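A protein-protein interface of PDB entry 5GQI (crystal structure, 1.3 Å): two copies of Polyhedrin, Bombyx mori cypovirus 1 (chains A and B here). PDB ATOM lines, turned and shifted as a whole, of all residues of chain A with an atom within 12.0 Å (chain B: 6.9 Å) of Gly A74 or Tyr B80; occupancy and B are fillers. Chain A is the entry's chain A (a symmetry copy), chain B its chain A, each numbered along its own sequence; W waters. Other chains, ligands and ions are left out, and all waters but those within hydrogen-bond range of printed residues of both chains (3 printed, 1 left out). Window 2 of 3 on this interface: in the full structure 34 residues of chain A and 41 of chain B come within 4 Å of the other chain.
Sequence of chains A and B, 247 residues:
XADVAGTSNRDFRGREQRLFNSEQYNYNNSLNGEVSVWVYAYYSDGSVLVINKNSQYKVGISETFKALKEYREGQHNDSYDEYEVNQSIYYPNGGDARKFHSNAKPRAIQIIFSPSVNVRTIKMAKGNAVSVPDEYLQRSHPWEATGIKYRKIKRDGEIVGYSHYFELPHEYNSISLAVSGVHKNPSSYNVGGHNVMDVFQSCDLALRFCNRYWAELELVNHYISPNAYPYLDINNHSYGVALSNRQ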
ATOM      1  N   ASP A  45      -6.716   8.026  12.102  1.00  0.00           N
ATOM      2  CA  ASP A  45      -7.145   8.963  11.006  1.00  0.00           C
ATOM      3  C   ASP A  45      -8.641   8.863  10.690  1.00  0.00           C
ATOM      4  O   ASP A  45      -9.101   9.508   9.717  1.00  0.00           O
ATOM      5  CB  ASP A  45      -6.285   8.727   9.721  1.00  0.00           C
ATOM      6  CG  ASP A  45      -6.475   7.405   9.093  1.00  0.00           C
ATOM      7  OD1 ASP A  45      -7.422   6.628   9.420  1.00  0.00           O
ATOM      8  OD2 ASP A  45      -5.661   7.125   8.187  1.00  0.00           O
ATOM      9  N   SER A  47     -10.340   6.311   9.693  1.00  0.00           N
ATOM     10  CA  SER A  47     -10.724   5.230   8.801  1.00  0.00           C
ATOM     11  C   SER A  47     -11.037   3.968   9.602  1.00  0.00           C
ATOM     12  O   SER A  47     -10.673   3.876  10.777  1.00  0.00           O
ATOM     13  CB  SER A  47      -9.648   5.074   7.662  1.00  0.00           C
ATOM     14  OG  SER A  47      -8.422   4.528   8.178  1.00  0.00           O
ATOM     15  N   GLU A  70      -3.522  -0.623   9.828  1.00  0.00           N
ATOM     16  CA  GLU A  70      -3.997   0.105   8.667  1.00  0.00           C
ATOM     17  C   GLU A  70      -3.093  -0.078   7.451  1.00  0.00           C
ATOM     18  O   GLU A  70      -1.863   0.128   7.553  1.00  0.00           O
ATOM     19  CB  GLU A  70      -4.041   1.596   9.036  1.00  0.00           C
ATOM     20  CG  GLU A  70      -4.679   2.474   7.913  1.00  0.00           C
ATOM     21  CD  GLU A  70      -4.799   3.927   8.280  1.00  0.00           C
ATOM     22  OE1 GLU A  70      -4.338   4.362   9.313  1.00  0.00           O
ATOM     23  OE2 GLU A  70      -5.395   4.675   7.430  1.00  0.00           O
ATOM     24  N   TYR A  71      -3.724  -0.310   6.301  1.00  0.00           N
ATOM     25  CA  TYR A  71      -2.984  -0.361   5.010  1.00  0.00           C
ATOM     26  C   TYR A  71      -3.803   0.479   4.022  1.00  0.00           C
ATOM     27  O   TYR A  71      -5.013   0.241   3.787  1.00  0.00           O
ATOM     28  CB  TYR A  71      -2.914  -1.867   4.556  1.00  0.00           C
ATOM     29  CG  TYR A  71      -2.194  -1.908   3.226  1.00  0.00           C
ATOM     30  CD1 TYR A  71      -0.812  -1.729   3.160  1.00  0.00           C
ATOM     31  CD2 TYR A  71      -2.908  -2.136   2.070  1.00  0.00           C
ATOM     32  CE1 TYR A  71      -0.141  -1.740   1.922  1.00  0.00           C
ATOM     33  CE2 TYR A  71      -2.276  -2.178   0.808  1.00  0.00           C
ATOM     34  CZ  TYR A  71      -0.909  -1.943   0.772  1.00  0.00           C
ATOM     35  OH  TYR A  71      -0.249  -2.016  -0.481  1.00  0.00           O
ATOM     36  N   ARG A  72      -3.180   1.506   3.487  1.00  0.00           N
ATOM     37  CA  ARG A  72      -3.828   2.427   2.533  1.00  0.00           C
ATOM     38  C   ARG A  72      -3.458   1.943   1.186  1.00  0.00           C
ATOM     39  O   ARG A  72      -2.382   2.162   0.689  1.00  0.00           O
ATOM     40  CB  ARG A  72      -3.317   3.849   2.785  1.00  0.00           C
ATOM     41  CG  ARG A  72      -3.486   4.317   4.241  1.00  0.00           C
ATOM     42  CD  ARG A  72      -3.256   5.805   4.410  1.00  0.00           C
ATOM     43  NE  ARG A  72      -1.946   6.205   3.954  1.00  0.00           N
ATOM     44  CZ  ARG A  72      -1.609   7.468   3.714  1.00  0.00           C
ATOM     45  NH1 ARG A  72      -2.487   8.439   3.969  1.00  0.00           N
ATOM     46  NH2 ARG A  72      -0.374   7.743   3.317  1.00  0.00           N
ATOM     47  N   GLU A  73      -4.444   1.324   0.515  1.00  0.00           N
ATOM     48  CA  GLU A  73      -4.168   0.843  -0.841  1.00  0.00           C
ATOM     49  C   GLU A  73      -3.760   1.989  -1.776  1.00  0.00           C
ATOM     50  O   GLU A  73      -4.468   3.037  -1.818  1.00  0.00           O
ATOM     51  CB  GLU A  73      -5.418   0.181  -1.473  1.00  0.00           C
ATOM     52  CG  GLU A  73      -5.814  -1.087  -0.782  1.00  0.00           C
ATOM     53  CD  GLU A  73      -7.114  -1.646  -1.407  1.00  0.00           C
ATOM     54  OE1 GLU A  73      -7.393  -1.494  -2.607  1.00  0.00           O
ATOM     55  OE2 GLU A  73      -7.937  -2.149  -0.657  1.00  0.00           O
ATOM     56  N   GLY A  74      -2.727   1.813  -2.556  1.00  0.00           N
ATOM     57  CA  GLY A  74      -2.323   2.786  -3.565  1.00  0.00           C
ATOM     58  C   GLY A  74      -1.661   4.057  -3.022  1.00  0.00           C
ATOM     59  O   GLY A  74      -1.399   4.978  -3.796  1.00  0.00           O
ATOM     60  N   GLN A  75      -1.385   4.124  -1.690  1.00  0.00           N
ATOM     61  CA  GLN A  75      -0.658   5.225  -1.060  1.00  0.00           C
ATOM     62  C   GLN A  75       0.549   4.722  -0.334  1.00  0.00           C
ATOM     63  O   GLN A  75       0.768   3.517  -0.194  1.00  0.00           O
ATOM     64  CB  GLN A  75      -1.591   5.934  -0.039  1.00  0.00           C
ATOM     65  CG  GLN A  75      -2.775   6.600  -0.735  1.00  0.00           C
ATOM     66  CD  GLN A  75      -3.699   7.337   0.269  1.00  0.00           C
ATOM     67  OE1 GLN A  75      -4.471   6.737   0.961  1.00  0.00           O
ATOM     68  NE2 GLN A  75      -3.462   8.640   0.456  1.00  0.00           N
ATOM     69  N   HIS A  76       1.397   5.685   0.052  1.00  0.00           N
ATOM     70  CA  HIS A  76       2.535   5.304   0.915  1.00  0.00           C
ATOM     71  C   HIS A  76       2.070   4.853   2.257  1.00  0.00           C
ATOM     72  O   HIS A  76       1.035   5.315   2.788  1.00  0.00           O
ATOM     73  CB  HIS A  76       3.527   6.471   1.025  1.00  0.00           C
ATOM     74  CG  HIS A  76       4.331   6.729  -0.233  1.00  0.00           C
ATOM     75  ND1 HIS A  76       5.092   5.758  -0.856  1.00  0.00           N
ATOM     76  CD2 HIS A  76       4.472   7.869  -0.979  1.00  0.00           C
ATOM     77  CE1 HIS A  76       5.687   6.298  -1.920  1.00  0.00           C
ATOM     78  NE2 HIS A  76       5.312   7.568  -2.006  1.00  0.00           N
ATOM     79  N   ASN A  77       2.795   3.881   2.820  1.00  0.00           N
ATOM     80  CA  ASN A  77       2.441   3.307   4.148  1.00  0.00           C
ATOM     81  C   ASN A  77       3.643   3.195   5.087  1.00  0.00           C
ATOM     82  O   ASN A  77       3.597   2.457   6.036  1.00  0.00           O
ATOM     83  CB  ASN A  77       1.796   1.898   3.958  1.00  0.00           C
ATOM     84  CG  ASN A  77       0.370   1.977   3.379  1.00  0.00           C
ATOM     85  OD1 ASN A  77      -0.545   2.300   4.084  1.00  0.00           O
ATOM     86  ND2 ASN A  77       0.249   1.712   2.076  1.00  0.00           N
ATOM     87  N   ASP A  78       4.710   3.917   4.791  1.00  0.00           N
ATOM     88  CA  ASP A  78       5.937   3.834   5.650  1.00  0.00           C
ATOM     89  C   ASP A  78       6.326   2.344   5.745  1.00  0.00           C
ATOM     90  O   ASP A  78       6.699   1.891   6.806  1.00  0.00           O
ATOM     91  CB  ASP A  78       5.718   4.377   7.131  1.00  0.00           C
ATOM     92  CG  ASP A  78       6.028   5.843   7.346  1.00  0.00           C
ATOM     93  OD1 ASP A  78       6.304   6.587   6.433  1.00  0.00           O
ATOM     94  OD2 ASP A  78       5.937   6.276   8.519  1.00  0.00           O
ATOM     95  N   SER A  79       6.305   1.609   4.630  1.00  0.00           N
ATOM     96  CA  SER A  79       6.377   0.154   4.709  1.00  0.00           C
ATOM     97  C   SER A  79       7.639  -0.404   5.372  1.00  0.00           C
ATOM     98  O   SER A  79       7.527  -1.353   6.188  1.00  0.00           O
ATOM     99  CB  SER A  79       6.103  -0.450   3.324  1.00  0.00           C
ATOM    100  OG  SER A  79       7.154  -0.190   2.401  1.00  0.00           O
ATOM    101  N   ASN A 211     -12.313  -4.394   3.585  1.00  0.00           N
ATOM    102  CA  ASN A 211     -12.140  -3.070   2.926  1.00  0.00           C
ATOM    103  C   ASN A 211     -11.903  -2.048   3.951  1.00  0.00           C
ATOM    104  O   ASN A 211     -12.425  -2.164   5.105  1.00  0.00           O
ATOM    105  CB  ASN A 211     -13.437  -2.680   2.145  1.00  0.00           C
ATOM    106  CG  ASN A 211     -13.259  -1.462   1.254  1.00  0.00           C
ATOM    107  OD1 ASN A 211     -12.284  -1.370   0.471  1.00  0.00           O
ATOM    108  ND2 ASN A 211     -14.113  -0.465   1.475  1.00  0.00           N
ATOM    109  N   ARG A 212     -11.146  -1.015   3.609  1.00  0.00           N
ATOM    110  CA  ARG A 212     -10.966   0.134   4.523  1.00  0.00           C
ATOM    111  C   ARG A 212     -11.819   1.310   4.031  1.00  0.00           C
ATOM    112  O   ARG A 212     -11.608   1.783   2.899  1.00  0.00           O
ATOM    113  CB  ARG A 212      -9.466   0.518   4.566  1.00  0.00           C
ATOM    114  CG  ARG A 212      -9.158   1.578   5.634  1.00  0.00           C
ATOM    115  CD  ARG A 212      -7.673   1.972   5.637  1.00  0.00           C
ATOM    116  NE  ARG A 212      -7.321   2.692   4.383  1.00  0.00           N
ATOM    117  CZ  ARG A 212      -7.362   4.020   4.221  1.00  0.00           C
ATOM    118  NH1 ARG A 212      -7.615   4.868   5.233  1.00  0.00           N
ATOM    119  NH2 ARG A 212      -7.094   4.515   2.972  1.00  0.00           N
ATOM    120  N   TYR A 213     -12.717   1.770   4.868  1.00  0.00           N
ATOM    121  CA  TYR A 213     -13.542   2.983   4.603  1.00  0.00           C
ATOM    122  C   TYR A 213     -12.875   4.144   5.299  1.00  0.00           C
ATOM    123  O   TYR A 213     -12.192   4.012   6.281  1.00  0.00           O
ATOM    124  CB  TYR A 213     -14.976   2.751   5.165  1.00  0.00           C
ATOM    125  CG  TYR A 213     -15.730   1.734   4.316  1.00  0.00           C
ATOM    126  CD1 TYR A 213     -16.355   2.134   3.148  1.00  0.00           C
ATOM    127  CD2 TYR A 213     -15.796   0.386   4.668  1.00  0.00           C
ATOM    128  CE1 TYR A 213     -17.003   1.235   2.289  1.00  0.00           C
ATOM    129  CE2 TYR A 213     -16.469  -0.541   3.853  1.00  0.00           C
ATOM    130  CZ  TYR A 213     -17.060  -0.104   2.717  1.00  0.00           C
ATOM    131  OH  TYR A 213     -17.715  -1.056   1.937  1.00  0.00           O
ATOM    132  N   TRP A 214     -13.150   5.314   4.805  1.00  0.00           N
ATOM    133  CA  TRP A 214     -12.436   6.522   5.291  1.00  0.00           C
ATOM    134  C   TRP A 214     -12.976   7.082   6.572  1.00  0.00           C
ATOM    135  O   TRP A 214     -12.317   7.899   7.173  1.00  0.00           O
ATOM    136  CB  TRP A 214     -12.418   7.660   4.216  1.00  0.00           C
ATOM    137  CG  TRP A 214     -11.607   7.386   3.030  1.00  0.00           C
ATOM    138  CD1 TRP A 214     -10.766   6.344   2.818  1.00  0.00           C
ATOM    139  CD2 TRP A 214     -11.613   8.217   1.856  1.00  0.00           C
ATOM    140  NE1 TRP A 214     -10.156   6.551   1.524  1.00  0.00           N
ATOM    141  CE2 TRP A 214     -10.690   7.681   0.966  1.00  0.00           C
ATOM    142  CE3 TRP A 214     -12.283   9.418   1.539  1.00  0.00           C
ATOM    143  CZ2 TRP A 214     -10.483   8.307  -0.373  1.00  0.00           C
ATOM    144  CZ3 TRP A 214     -12.059  10.031   0.265  1.00  0.00           C
ATOM    145  CH2 TRP A 214     -11.185   9.430  -0.667  1.00  0.00           C
ATOM    146  N   ALA A 215     -14.219   6.759   6.931  1.00  0.00           N
ATOM    147  CA  ALA A 215     -14.855   7.417   8.079  1.00  0.00           C
ATOM    148  C   ALA A 215     -16.009   6.537   8.548  1.00  0.00           C
ATOM    149  O   ALA A 215     -16.597   5.812   7.719  1.00  0.00           O
ATOM    150  CB  ALA A 215     -15.426   8.761   7.631  1.00  0.00           C
ATOM    151  N   GLU A 218     -18.956   7.124   6.372  1.00  0.00           N
ATOM    152  CA  GLU A 218     -18.954   6.419   5.101  1.00  0.00           C
ATOM    153  C   GLU A 218     -19.247   4.938   5.282  1.00  0.00           C
ATOM    154  O   GLU A 218     -19.992   4.295   4.489  1.00  0.00           O
ATOM    155  CB  GLU A 218     -17.566   6.569   4.459  1.00  0.00           C
ATOM    156  CG  GLU A 218     -17.462   5.977   3.040  1.00  0.00           C
ATOM    157  CD  GLU A 218     -16.102   6.321   2.482  1.00  0.00           C
ATOM    158  OE1 GLU A 218     -15.147   5.562   2.863  1.00  0.00           O
ATOM    159  OE2 GLU A 218     -15.937   7.299   1.708  1.00  0.00           O
ATOM    160  N   ASN B  77      -0.368  -1.530 -11.561  1.00  0.00           N
ATOM    161  CA  ASN B  77      -1.755  -2.072 -11.514  1.00  0.00           C
ATOM    162  C   ASN B  77      -2.805  -0.995 -11.243  1.00  0.00           C
ATOM    163  O   ASN B  77      -3.896  -1.306 -10.843  1.00  0.00           O
ATOM    164  CB  ASN B  77      -1.851  -3.180 -10.417  1.00  0.00           C
ATOM    165  CG  ASN B  77      -1.134  -4.479 -10.830  1.00  0.00           C
ATOM    166  OD1 ASN B  77      -1.646  -5.221 -11.622  1.00  0.00           O
ATOM    167  ND2 ASN B  77       0.072  -4.683 -10.293  1.00  0.00           N
ATOM    168  N   ASP B  78      -2.448   0.262 -11.448  1.00  0.00           N
ATOM    169  CA  ASP B  78      -3.417   1.374 -11.174  1.00  0.00           C
ATOM    170  C   ASP B  78      -3.908   1.202  -9.722  1.00  0.00           C
ATOM    171  O   ASP B  78      -5.079   1.383  -9.462  1.00  0.00           O
ATOM    172  CB  ASP B  78      -4.693   1.359 -12.126  1.00  0.00           C
ATOM    173  CG  ASP B  78      -4.575   2.173 -13.396  1.00  0.00           C
ATOM    174  OD1 ASP B  78      -3.540   2.702 -13.733  1.00  0.00           O
ATOM    175  OD2 ASP B  78      -5.593   2.239 -14.125  1.00  0.00           O
ATOM    176  N   SER B  79      -3.008   0.923  -8.774  1.00  0.00           N
ATOM    177  CA  SER B  79      -3.445   0.467  -7.459  1.00  0.00           C
ATOM    178  C   SER B  79      -4.343   1.442  -6.693  1.00  0.00           C
ATOM    179  O   SER B  79      -5.350   0.994  -6.091  1.00  0.00           O
ATOM    180  CB  SER B  79      -2.228   0.000  -6.647  1.00  0.00           C
ATOM    181  OG  SER B  79      -1.376   1.078  -6.277  1.00  0.00           O
ATOM    182  N   TYR B  80      -4.064   2.736  -6.790  1.00  0.00           N
ATOM    183  CA  TYR B  80      -4.942   3.703  -6.157  1.00  0.00           C
ATOM    184  C   TYR B  80      -6.287   3.823  -6.899  1.00  0.00           C
ATOM    185  O   TYR B  80      -7.362   3.779  -6.278  1.00  0.00           O
ATOM    186  CB  TYR B  80      -4.243   5.115  -6.003  1.00  0.00           C
ATOM    187  CG  TYR B  80      -5.216   5.898  -5.187  1.00  0.00           C
ATOM    188  CD1 TYR B  80      -5.202   5.740  -3.771  1.00  0.00           C
ATOM    189  CD2 TYR B  80      -6.195   6.783  -5.744  1.00  0.00           C
ATOM    190  CE1 TYR B  80      -6.156   6.357  -2.988  1.00  0.00           C
ATOM    191  CE2 TYR B  80      -7.168   7.334  -4.926  1.00  0.00           C
ATOM    192  CZ  TYR B  80      -7.135   7.093  -3.585  1.00  0.00           C
ATOM    193  OH  TYR B  80      -8.124   7.565  -2.749  1.00  0.00           O
ATOM    194  N   ASP B  81      -6.243   3.995  -8.232  1.00  0.00           N
ATOM    195  CA  ASP B  81      -7.528   4.039  -8.943  1.00  0.00           C
ATOM    196  C   ASP B  81      -8.363   2.800  -8.713  1.00  0.00           C
ATOM    197  O   ASP B  81      -9.576   2.905  -8.674  1.00  0.00           O
ATOM    198  CB  ASP B  81      -7.256   4.226 -10.451  1.00  0.00           C
ATOM    199  CG  ASP B  81      -8.487   4.802 -11.198  1.00  0.00           C
ATOM    200  OD1 ASP B  81      -9.080   5.747 -10.680  1.00  0.00           O
ATOM    201  OD2 ASP B  81      -8.875   4.221 -12.246  1.00  0.00           O
ATOM    202  N   GLU B  82      -7.710   1.629  -8.542  1.00  0.00           N
ATOM    203  CA  GLU B  82      -8.440   0.368  -8.360  1.00  0.00           C
ATOM    204  C   GLU B  82      -9.066   0.271  -6.953  1.00  0.00           C
ATOM    205  O   GLU B  82     -10.120  -0.384  -6.812  1.00  0.00           O
ATOM    206  CB  GLU B  82      -7.571  -0.866  -8.681  1.00  0.00           C
ATOM    207  CG  GLU B  82      -7.323  -0.936 -10.201  1.00  0.00           C
ATOM    208  CD  GLU B  82      -8.538  -1.271 -11.052  1.00  0.00           C
ATOM    209  OE1 GLU B  82      -9.458  -1.893 -10.520  1.00  0.00           O
ATOM    210  OE2 GLU B  82      -8.618  -0.813 -12.244  1.00  0.00           O
ATOM    211  N   TYR B  83      -8.453   0.913  -5.938  1.00  0.00           N
ATOM    212  CA  TYR B  83      -9.183   1.080  -4.657  1.00  0.00           C
ATOM    213  C   TYR B  83     -10.478   1.918  -4.936  1.00  0.00           C
ATOM    214  O   TYR B  83     -11.577   1.562  -4.400  1.00  0.00           O
ATOM    215  CB  TYR B  83      -8.271   1.816  -3.647  1.00  0.00           C
ATOM    216  CG  TYR B  83      -9.012   2.234  -2.398  1.00  0.00           C
ATOM    217  CD1 TYR B  83      -9.227   1.375  -1.340  1.00  0.00           C
ATOM    218  CD2 TYR B  83      -9.484   3.549  -2.289  1.00  0.00           C
ATOM    219  CE1 TYR B  83      -9.994   1.791  -0.163  1.00  0.00           C
ATOM    220  CE2 TYR B  83     -10.240   3.967  -1.200  1.00  0.00           C
ATOM    221  CZ  TYR B  83     -10.444   3.096  -0.150  1.00  0.00           C
ATOM    222  OH  TYR B  83     -11.156   3.523   0.938  1.00  0.00           O
ATOM    223  N   GLU B  84     -10.380   2.995  -5.670  1.00  0.00           N
ATOM    224  CA  GLU B  84     -11.581   3.816  -5.953  1.00  0.00           C
ATOM    225  C   GLU B  84     -12.588   3.041  -6.803  1.00  0.00           C
ATOM    226  O   GLU B  84     -13.799   3.133  -6.587  1.00  0.00           O
ATOM    227  CB  GLU B  84     -11.146   5.101  -6.695  1.00  0.00           C
ATOM    228  CG  GLU B  84     -10.319   6.033  -5.859  1.00  0.00           C
ATOM    229  CD  GLU B  84     -11.142   6.753  -4.745  1.00  0.00           C
ATOM    230  OE1 GLU B  84     -12.379   6.625  -4.752  1.00  0.00           O
ATOM    231  OE2 GLU B  84     -10.489   7.394  -3.875  1.00  0.00           O
ATOM    232  N   VAL B  85     -12.121   2.198  -7.717  1.00  0.00           N
ATOM    233  CA  VAL B  85     -13.053   1.280  -8.426  1.00  0.00           C
ATOM    234  C   VAL B  85     -13.780   0.413  -7.424  1.00  0.00           C
ATOM    235  O   VAL B  85     -15.017   0.319  -7.537  1.00  0.00           O
ATOM    236  CB  VAL B  85     -12.250   0.361  -9.417  1.00  0.00           C
ATOM    237  CG1 VAL B  85     -13.032  -0.854  -9.864  1.00  0.00           C
ATOM    238  CG2 VAL B  85     -11.737   1.141 -10.604  1.00  0.00           C
ATOM    239  N   ASP B  96     -14.356   7.392  -6.595  1.00  0.00           N
ATOM    240  CA  ASP B  96     -13.993   8.479  -7.542  1.00  0.00           C
ATOM    241  C   ASP B  96     -12.967   7.982  -8.495  1.00  0.00           C
ATOM    242  O   ASP B  96     -11.860   8.565  -8.659  1.00  0.00           O
ATOM    243  CB  ASP B  96     -13.542   9.714  -6.729  1.00  0.00           C
ATOM    244  CG  ASP B  96     -14.808  10.512  -6.267  1.00  0.00           C
ATOM    245  OD1 ASP B  96     -15.614  10.975  -7.115  1.00  0.00           O
ATOM    246  OD2 ASP B  96     -15.148  10.633  -5.079  1.00  0.00           O
ATOM    247  N   ALA B  97     -13.230   6.853  -9.150  1.00  0.00           N
ATOM    248  CA  ALA B  97     -12.272   6.263 -10.110  1.00  0.00           C
ATOM    249  C   ALA B  97     -12.271   7.031 -11.414  1.00  0.00           C
ATOM    250  O   ALA B  97     -13.225   7.707 -11.803  1.00  0.00           O
ATOM    251  CB  ALA B  97     -12.639   4.814 -10.345  1.00  0.00           C
HETATM  252  O   HOH W   1      -6.242  -1.555  -5.016  1.00  0.00           O
HETATM  253  O   HOH W   2     -13.340   5.174   0.737  1.00  0.00           O
HETATM  254  O   HOH W   3      -7.955   6.084  -0.115  1.00  0.00           O
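Among the printed residues, pairs that only touch across the chains: Gly A74 with Ser B79 (3.3 Å), Glu A73 with Tyr B80 (3.4 Å), Trp A214 with Tyr B80 (3.4 Å), Glu A73 with Tyr B83 (3.6 Å), Gly A74 with Tyr B80 (3.6 Å), Trp A214 with Glu B84 (3.6 Å), Asn A211 with Tyr B83 (3.95 Å) and Gln A75 with Tyr B80 (3.98 Å).
OH of Tyr B83 is in hydrogen-bond range of NE1 of Trp A214 (3.2 Å).
O of Arg A212 sits at hydrogen-bond distance from OH of Tyr B83 (2.7 Å).
OG of Ser A47 sits at hydrogen-bond distance from NH1 of Arg A212 (3.1 Å).
The side-chain carboxylate (OE1) of Glu B84 lies within hydrogen-bond range of the backbone NH (N) of Asp B96.
OE2 of Glu B84 lies within hydrogen-bond range of OH of Tyr B80, 2.6 Å away.
The backbone NH (N) of Trp A214 sits at hydrogen-bond distance from the side-chain carboxylate (OE1) of Glu A218 (2.8 Å).
The backbone carbonyl oxygen (O) of Tyr A71 lies within hydrogen-bond range of the guanidinium group (NE) of Arg A212, at 3.4 Å.
OE2 of Glu A70 lies within salt-bridge range of NH1 of Arg A212 (3.1 Å).
Printed residues of chain B within 4 Å of Gly A74: Ser B79 and Tyr B80.
Printed residues of chain A within 4 Å of Tyr B80: Glu A73 (3.4 Å), Gly A74 (3.6 Å), Gln A75 (3.98 Å) and Trp A214 (3.4 Å).
No residue of chain A comes within 4 Å of Asp B78.
No residue of chain A comes within 4 Å of Asp B81.
No residue of chain A comes within 4 Å of Glu B82.
Tyr B83 touches just these residues of chain A: Glu A73 (3.6 Å), Asn A211 (3.95 Å), Arg A212 (2.7 Å) and Trp A214 (3.2 Å).
Of the printed residues of chain B, Glu A73 touches Tyr B80 and Tyr B83.
Printed residues of chain B within 4 Å of Trp A214: Tyr B80, Tyr B83 and Glu B84.
Of the printed residues of chain A, Ser B79 touches Gly A74.
Printed residues of chain B within 4 Å of Gln A75: Tyr B80 (3.98 Å).
Printed residues of chain B within 4 Å of Asn A211: Tyr B83 (3.95 Å).
Val B85 touches none of the printed residues of chain A.
His A76 touches none of the printed residues of chain B.
The nearest printed residue of chain A that does not touch Tyr B80 is Arg A212 (6.3 Å).
The nearest printed residue of chain B that does not touch Arg A212 is Tyr B80 (6.3 Å).
Water W1 lies within hydrogen-bond range of the side-chain carboxylate of Glu A73 (2.7 Å), the backbone carbonyl oxygen of Ser B79 (2.9 Å) and the backbone NH of Tyr B83 (3.4 Å).
Water W2 lies within hydrogen-bond range of the side-chain hydroxyl (OH) of Tyr B83 (2.7 Å) and the side-chain carboxylate (OE1) of Glu A218 (2.8 Å).
Water W3 bridges NE1 of Trp A214 (2.8 Å) and OH of Tyr B80 (3.0 Å).
3 positions are printed for both chains.
Of the 10 pairs that touch across the chains among the printed residues, none has its exchanged pair printed and touching as well.
Hydrophobic or aromatic side chains of chain A within 4 Å of the printed part of chain B: Trp A214.
Hydrophobic or aromatic side chains of chain B within 4 Å of the printed part of chain A: Tyr B80 and Tyr B83.
Among the printed residues, 10 pairs touch across the chains.
Among the printed residues, no Asp or Glu carboxylate lies within 4 Å of a Lys or Arg side-chain nitrogen of the other chain.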
